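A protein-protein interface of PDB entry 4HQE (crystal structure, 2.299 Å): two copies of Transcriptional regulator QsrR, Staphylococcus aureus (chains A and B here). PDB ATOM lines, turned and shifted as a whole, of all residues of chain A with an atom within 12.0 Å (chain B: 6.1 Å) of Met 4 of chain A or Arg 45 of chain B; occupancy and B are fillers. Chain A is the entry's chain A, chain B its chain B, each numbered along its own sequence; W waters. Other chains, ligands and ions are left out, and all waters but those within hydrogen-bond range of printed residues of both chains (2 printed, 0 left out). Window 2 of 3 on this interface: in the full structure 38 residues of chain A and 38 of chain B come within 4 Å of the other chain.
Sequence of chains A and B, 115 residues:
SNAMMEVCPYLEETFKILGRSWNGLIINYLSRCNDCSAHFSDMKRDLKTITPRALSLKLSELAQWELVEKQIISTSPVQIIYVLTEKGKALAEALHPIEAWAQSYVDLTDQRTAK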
ATOM      1  N   MET A   4      23.408  -0.978   8.706  1.00  0.00           N
ATOM      2  CA  MET A   4      24.586  -1.761   8.324  1.00  0.00           C
ATOM      3  C   MET A   4      24.642  -3.087   9.102  1.00  0.00           C
ATOM      4  O   MET A   4      25.252  -4.068   8.654  1.00  0.00           O
ATOM      5  CB  MET A   4      25.861  -0.954   8.566  1.00  0.00           C
ATOM      6  CG  MET A   4      27.057  -1.401   7.738  1.00  0.00           C
ATOM      7  SD  MET A   4      27.161  -0.577   6.125  1.00  0.00           S
ATOM      8  CE  MET A   4      27.156   1.155   6.611  1.00  0.00           C
ATOM      9  N   MET A   5      23.999  -3.092  10.272  1.00  0.00           N
ATOM     10  CA  MET A   5      23.822  -4.280  11.103  1.00  0.00           C
ATOM     11  C   MET A   5      22.700  -3.949  12.083  1.00  0.00           C
ATOM     12  O   MET A   5      22.884  -3.988  13.303  1.00  0.00           O
ATOM     13  CB  MET A   5      25.111  -4.604  11.855  1.00  0.00           C
ATOM     14  CG  MET A   5      25.827  -5.861  11.370  1.00  0.00           C
ATOM     15  SD  MET A   5      25.252  -7.328  12.235  1.00  0.00           S
ATOM     16  CE  MET A   5      25.600  -6.883  13.947  1.00  0.00           C
ATOM     17  N   GLU A   6      21.536  -3.629  11.527  1.00  0.00           N
ATOM     18  CA  GLU A   6      20.478  -2.930  12.252  1.00  0.00           C
ATOM     19  C   GLU A   6      19.973  -3.651  13.497  1.00  0.00           C
ATOM     20  O   GLU A   6      20.070  -4.873  13.602  1.00  0.00           O
ATOM     21  CB  GLU A   6      19.301  -2.629  11.304  1.00  0.00           C
ATOM     22  CG  GLU A   6      18.558  -1.313  11.585  1.00  0.00           C
ATOM     23  CD  GLU A   6      19.335  -0.070  11.125  1.00  0.00           C
ATOM     24  OE1 GLU A   6      18.710   0.835  10.519  1.00  0.00           O
ATOM     25  OE2 GLU A   6      20.564   0.016  11.381  1.00  0.00           O
ATOM     26  N   VAL A   7      19.436  -2.865  14.430  1.00  0.00           N
ATOM     27  CA  VAL A   7      18.856  -3.367  15.668  1.00  0.00           C
ATOM     28  C   VAL A   7      17.340  -3.524  15.507  1.00  0.00           C
ATOM     29  O   VAL A   7      16.671  -2.617  14.999  1.00  0.00           O
ATOM     30  CB  VAL A   7      19.086  -2.365  16.806  1.00  0.00           C
ATOM     31  CG1 VAL A   7      18.615  -2.938  18.136  1.00  0.00           C
ATOM     32  CG2 VAL A   7      20.551  -1.957  16.866  1.00  0.00           C
ATOM     33  N   CYS A   8      16.808  -4.664  15.942  1.00  0.00           N
ATOM     34  CA  CYS A   8      15.370  -4.893  15.971  1.00  0.00           C
ATOM     35  C   CYS A   8      14.644  -3.800  16.767  1.00  0.00           C
ATOM     36  O   CYS A   8      14.977  -3.541  17.939  1.00  0.00           O
ATOM     37  CB  CYS A   8      15.070  -6.255  16.581  1.00  0.00           C
ATOM     38  SG  CYS A   8      13.308  -6.684  16.635  1.00  0.00           S
ATOM     39  N   GLU A  12      14.256  -3.160  20.747  1.00  0.00           N
ATOM     40  CA  GLU A  12      14.537  -1.813  21.228  1.00  0.00           C
ATOM     41  C   GLU A  12      13.409  -1.263  22.112  1.00  0.00           C
ATOM     42  O   GLU A  12      13.650  -0.678  23.177  1.00  0.00           O
ATOM     43  CB  GLU A  12      14.733  -0.894  20.034  1.00  0.00           C
ATOM     44  CG  GLU A  12      15.237   0.439  20.429  1.00  0.00           C
ATOM     45  CD  GLU A  12      15.818   1.178  19.256  1.00  0.00           C
ATOM     46  OE1 GLU A  12      16.167   2.369  19.448  1.00  0.00           O
ATOM     47  OE2 GLU A  12      15.916   0.561  18.156  1.00  0.00           O
ATOM     48  N   TYR B  29      23.767  -6.340  20.136  1.00  0.00           N
ATOM     49  CA  TYR B  29      24.380  -5.902  18.888  1.00  0.00           C
ATOM     50  C   TYR B  29      25.744  -6.587  18.676  1.00  0.00           C
ATOM     51  O   TYR B  29      26.062  -7.032  17.570  1.00  0.00           O
ATOM     52  CB  TYR B  29      24.549  -4.378  18.893  1.00  0.00           C
ATOM     53  CG  TYR B  29      25.360  -3.832  17.733  1.00  0.00           C
ATOM     54  CD1 TYR B  29      26.731  -3.587  17.862  1.00  0.00           C
ATOM     55  CD2 TYR B  29      24.759  -3.555  16.511  1.00  0.00           C
ATOM     56  CE1 TYR B  29      27.485  -3.082  16.783  1.00  0.00           C
ATOM     57  CE2 TYR B  29      25.493  -3.055  15.444  1.00  0.00           C
ATOM     58  CZ  TYR B  29      26.851  -2.819  15.586  1.00  0.00           C
ATOM     59  OH  TYR B  29      27.575  -2.321  14.529  1.00  0.00           O
ATOM     60  N   PHE B  40      33.888   1.506  17.965  1.00  0.00           N
ATOM     61  CA  PHE B  40      33.042   2.518  18.589  1.00  0.00           C
ATOM     62  C   PHE B  40      32.046   3.126  17.588  1.00  0.00           C
ATOM     63  O   PHE B  40      30.846   3.200  17.860  1.00  0.00           O
ATOM     64  CB  PHE B  40      33.932   3.613  19.162  1.00  0.00           C
ATOM     65  CG  PHE B  40      33.218   4.564  20.053  1.00  0.00           C
ATOM     66  CD1 PHE B  40      33.157   4.333  21.420  1.00  0.00           C
ATOM     67  CD2 PHE B  40      32.595   5.693  19.530  1.00  0.00           C
ATOM     68  CE1 PHE B  40      32.488   5.216  22.261  1.00  0.00           C
ATOM     69  CE2 PHE B  40      31.915   6.586  20.371  1.00  0.00           C
ATOM     70  CZ  PHE B  40      31.868   6.344  21.735  1.00  0.00           C
ATOM     71  N   SER B  41      32.569   3.537  16.435  1.00  0.00           N
ATOM     72  CA  SER B  41      31.781   4.049  15.313  1.00  0.00           C
ATOM     73  C   SER B  41      30.764   3.077  14.716  1.00  0.00           C
ATOM     74  O   SER B  41      29.800   3.524  14.109  1.00  0.00           O
ATOM     75  CB  SER B  41      32.706   4.514  14.178  1.00  0.00           C
ATOM     76  OG  SER B  41      33.842   5.185  14.706  1.00  0.00           O
ATOM     77  N   ASP B  42      30.981   1.768  14.833  1.00  0.00           N
ATOM     78  CA  ASP B  42      29.971   0.831  14.320  1.00  0.00           C
ATOM     79  C   ASP B  42      28.749   0.899  15.222  1.00  0.00           C
ATOM     80  O   ASP B  42      27.618   1.047  14.754  1.00  0.00           O
ATOM     81  CB  ASP B  42      30.477  -0.625  14.267  1.00  0.00           C
ATOM     82  CG  ASP B  42      31.634  -0.824  13.293  1.00  0.00           C
ATOM     83  OD1 ASP B  42      31.617  -0.196  12.216  1.00  0.00           O
ATOM     84  OD2 ASP B  42      32.562  -1.610  13.608  1.00  0.00           O
ATOM     85  N   MET B  43      28.997   0.790  16.525  1.00  0.00           N
ATOM     86  CA  MET B  43      27.931   0.800  17.518  1.00  0.00           C
ATOM     87  C   MET B  43      27.172   2.127  17.514  1.00  0.00           C
ATOM     88  O   MET B  43      25.935   2.134  17.570  1.00  0.00           O
ATOM     89  CB  MET B  43      28.489   0.492  18.911  1.00  0.00           C
ATOM     90  CG  MET B  43      28.982  -0.935  19.062  1.00  0.00           C
ATOM     91  SD  MET B  43      29.600  -1.333  20.705  1.00  0.00           S
ATOM     92  CE  MET B  43      31.299  -0.728  20.554  1.00  0.00           C
ATOM     93  N   LYS B  44      27.898   3.246  17.425  1.00  0.00           N
ATOM     94  CA  LYS B  44      27.225   4.545  17.340  1.00  0.00           C
ATOM     95  C   LYS B  44      26.339   4.612  16.094  1.00  0.00           C
ATOM     96  O   LYS B  44      25.156   4.960  16.188  1.00  0.00           O
ATOM     97  CB  LYS B  44      28.205   5.719  17.376  1.00  0.00           C
ATOM     98  CG  LYS B  44      27.510   7.063  17.670  1.00  0.00           C
ATOM     99  CD  LYS B  44      28.495   8.221  17.690  1.00  0.00           C
ATOM    100  CE  LYS B  44      28.008   9.371  16.816  1.00  0.00           C
ATOM    101  NZ  LYS B  44      29.134  10.287  16.448  1.00  0.00           N
ATOM    102  N   ARG B  45      26.899   4.252  14.939  1.00  0.00           N
ATOM    103  CA  ARG B  45      26.113   4.206  13.714  1.00  0.00           C
ATOM    104  C   ARG B  45      24.817   3.347  13.803  1.00  0.00           C
ATOM    105  O   ARG B  45      23.730   3.823  13.464  1.00  0.00           O
ATOM    106  CB  ARG B  45      26.972   3.745  12.532  1.00  0.00           C
ATOM    107  CG  ARG B  45      26.215   3.725  11.182  1.00  0.00           C
ATOM    108  CD  ARG B  45      26.905   2.837  10.146  1.00  0.00           C
ATOM    109  NE  ARG B  45      27.168   1.493  10.666  1.00  0.00           N
ATOM    110  CZ  ARG B  45      28.363   0.903  10.640  1.00  0.00           C
ATOM    111  NH1 ARG B  45      29.405   1.532  10.100  1.00  0.00           N
ATOM    112  NH2 ARG B  45      28.516  -0.322  11.137  1.00  0.00           N
ATOM    113  N   ASP B  46      24.930   2.099  14.257  1.00  0.00           N
ATOM    114  CA  ASP B  46      23.820   1.154  14.147  1.00  0.00           C
ATOM    115  C   ASP B  46      22.831   1.216  15.315  1.00  0.00           C
ATOM    116  O   ASP B  46      21.702   0.739  15.193  1.00  0.00           O
ATOM    117  CB  ASP B  46      24.322  -0.284  13.924  1.00  0.00           C
ATOM    118  CG  ASP B  46      25.253  -0.406  12.722  1.00  0.00           C
ATOM    119  OD1 ASP B  46      26.075  -1.351  12.698  1.00  0.00           O
ATOM    120  OD2 ASP B  46      25.167   0.434  11.797  1.00  0.00           O
ATOM    121  N   LEU B  47      23.251   1.798  16.435  1.00  0.00           N
ATOM    122  CA  LEU B  47      22.357   2.030  17.567  1.00  0.00           C
ATOM    123  C   LEU B  47      21.521   3.304  17.316  1.00  0.00           C
ATOM    124  O   LEU B  47      20.508   3.542  17.998  1.00  0.00           O
ATOM    125  CB  LEU B  47      23.151   2.143  18.875  1.00  0.00           C
ATOM    126  CG  LEU B  47      23.230   0.980  19.883  1.00  0.00           C
ATOM    127  CD1 LEU B  47      22.630  -0.325  19.379  1.00  0.00           C
ATOM    128  CD2 LEU B  47      24.651   0.757  20.362  1.00  0.00           C
ATOM    129  N   LYS B  48      21.975   4.114  16.350  1.00  0.00           N
ATOM    130  CA  LYS B  48      21.187   5.210  15.741  1.00  0.00           C
ATOM    131  C   LYS B  48      21.018   6.448  16.622  1.00  0.00           C
ATOM    132  O   LYS B  48      21.357   7.557  16.206  1.00  0.00           O
ATOM    133  CB  LYS B  48      19.809   4.711  15.247  1.00  0.00           C
ATOM    134  CG  LYS B  48      19.884   3.640  14.155  1.00  0.00           C
ATOM    135  CD  LYS B  48      18.549   2.913  13.973  1.00  0.00           C
ATOM    136  CE  LYS B  48      18.266   1.955  15.133  1.00  0.00           C
ATOM    137  NZ  LYS B  48      17.368   0.823  14.731  1.00  0.00           N
ATOM    138  N   THR B  49      20.509   6.260  17.840  1.00  0.00           N
ATOM    139  CA  THR B  49      20.176   7.402  18.687  1.00  0.00           C
ATOM    140  C   THR B  49      20.988   7.506  19.972  1.00  0.00           C
ATOM    141  O   THR B  49      20.644   8.307  20.860  1.00  0.00           O
ATOM    142  CB  THR B  49      18.670   7.423  19.044  1.00  0.00           C
ATOM    143  OG1 THR B  49      18.325   6.219  19.751  1.00  0.00           O
ATOM    144  CG2 THR B  49      17.806   7.557  17.765  1.00  0.00           C
HETATM  145  O   HOH W   1      17.023   4.552  18.239  1.00  0.00           O
HETATM  146  O   HOH W   2      18.873   1.556  19.127  1.00  0.00           O
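No position is printed for both chains. Of the 9 pairs that touch across the chains among the printed residues, none has its exchanged pair printed and touching as well.
The side-chain amino group (NZ) of Lys 48 of chain B is in salt-bridge range of the side-chain carboxylate (OE2) of Glu 12 of chain A (3.7 Å).
Met 4 of chain A touches just these residues of chain B: Arg 45 and Asp 46. Printed residues of chain B within 4 Å of Met 5 of chain A: Tyr 29 and Asp 46. Of the printed residues of chain B, Glu 6 of chain A touches Lys 48. Of the printed residues of chain A, Tyr 29 of chain B touches Met 5 (3.5 Å). Phe 40 of chain B touches none of the printed residues of chain A. No residue of chain A comes within 4 Å of Ser 41 of chain B. No residue of chain A comes within 4 Å of Asp 42 of chain B. No residue of chain A comes within 4 Å of Lys 44 of chain B. Arg 45 of chain B touches just one residue of chain A: Met 4. Of the printed residues of chain A, Lys 48 of chain B touches Glu 6 (3.98 Å), Val 7 (3.5 Å) and Glu 12 (3.7 Å). The nearest printed residue of chain B that does not touch Glu 12 of chain A is Thr 49 of chain B (4.4 Å).
Water W1 lies within hydrogen-bond range of the side-chain hydroxyl of Thr 49 of chain B (2.6 Å) and the side-chain carboxylate of Glu 12 of chain A (2.6 Å). Water W2 lies within hydrogen-bond range of the backbone carbonyl oxygen of Leu 47 of chain B (2.8 Å) and the side-chain carboxylate of Glu 12 of chain A (2.8 Å).
The backbone carbonyl oxygen (O) of Asp 42 of chain B lies close to the side-chain hydroxyl (OH) of Tyr 29 of chain B. OH of Tyr 29 of chain B is in hydrogen-bond range of OD1 of Asp 46 of chain B (2.6 Å). OD1 of Asp 42 of chain B is in salt-bridge range of NH2 of Arg 45 of chain B, 3.3 Å away. The side-chain carboxylate (OD2) of Asp 46 of chain B is in salt-bridge range of the guanidinium group (NE) of Arg 45 of chain B (2.5 Å).
CB of Met 4 of chain A touches NE of Arg 45 of chain B, at 3.5 Å. OD2 of Asp 46 of chain B touches CB of Met 4 of chain A, at 3.6 Å. CE2 of Tyr 29 of chain B touches O of Met 5 of chain A (3.5 Å). Asp 46 of chain B touches Met 5 of chain A. Glu 6 of chain A touches Lys 48 of chain B. Val 7 of chain A touches Asp 46 of chain B (CG2 to O, 3.4 Å). Leu 47 of chain B touches Val 7 of chain A (CD1 to CG2, 3.6 Å). Val 7 of chain A touches Lys 48 of chain B.
Hydrophobic or aromatic side chains of chain A within 4 Å of the printed part of chain B: Met 4, Met 5 and Val 7. Printed residues of chain B that touch a printed residue of chain A: Tyr 29, Arg 45, Asp 46, Leu 47 and Lys 48. Hydrophobic or aromatic side chains of chain B within 4 Å of the printed part of chain A: Tyr 29 and Leu 47. Among the printed residues, 9 pairs touch across the chains. Among the printed residues, Asp or Glu carboxylates within 4 Å of a Lys or Arg side-chain nitrogen of the other chain: Glu 12 of chain A with Lys 48 of chain B (3.7 Å).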
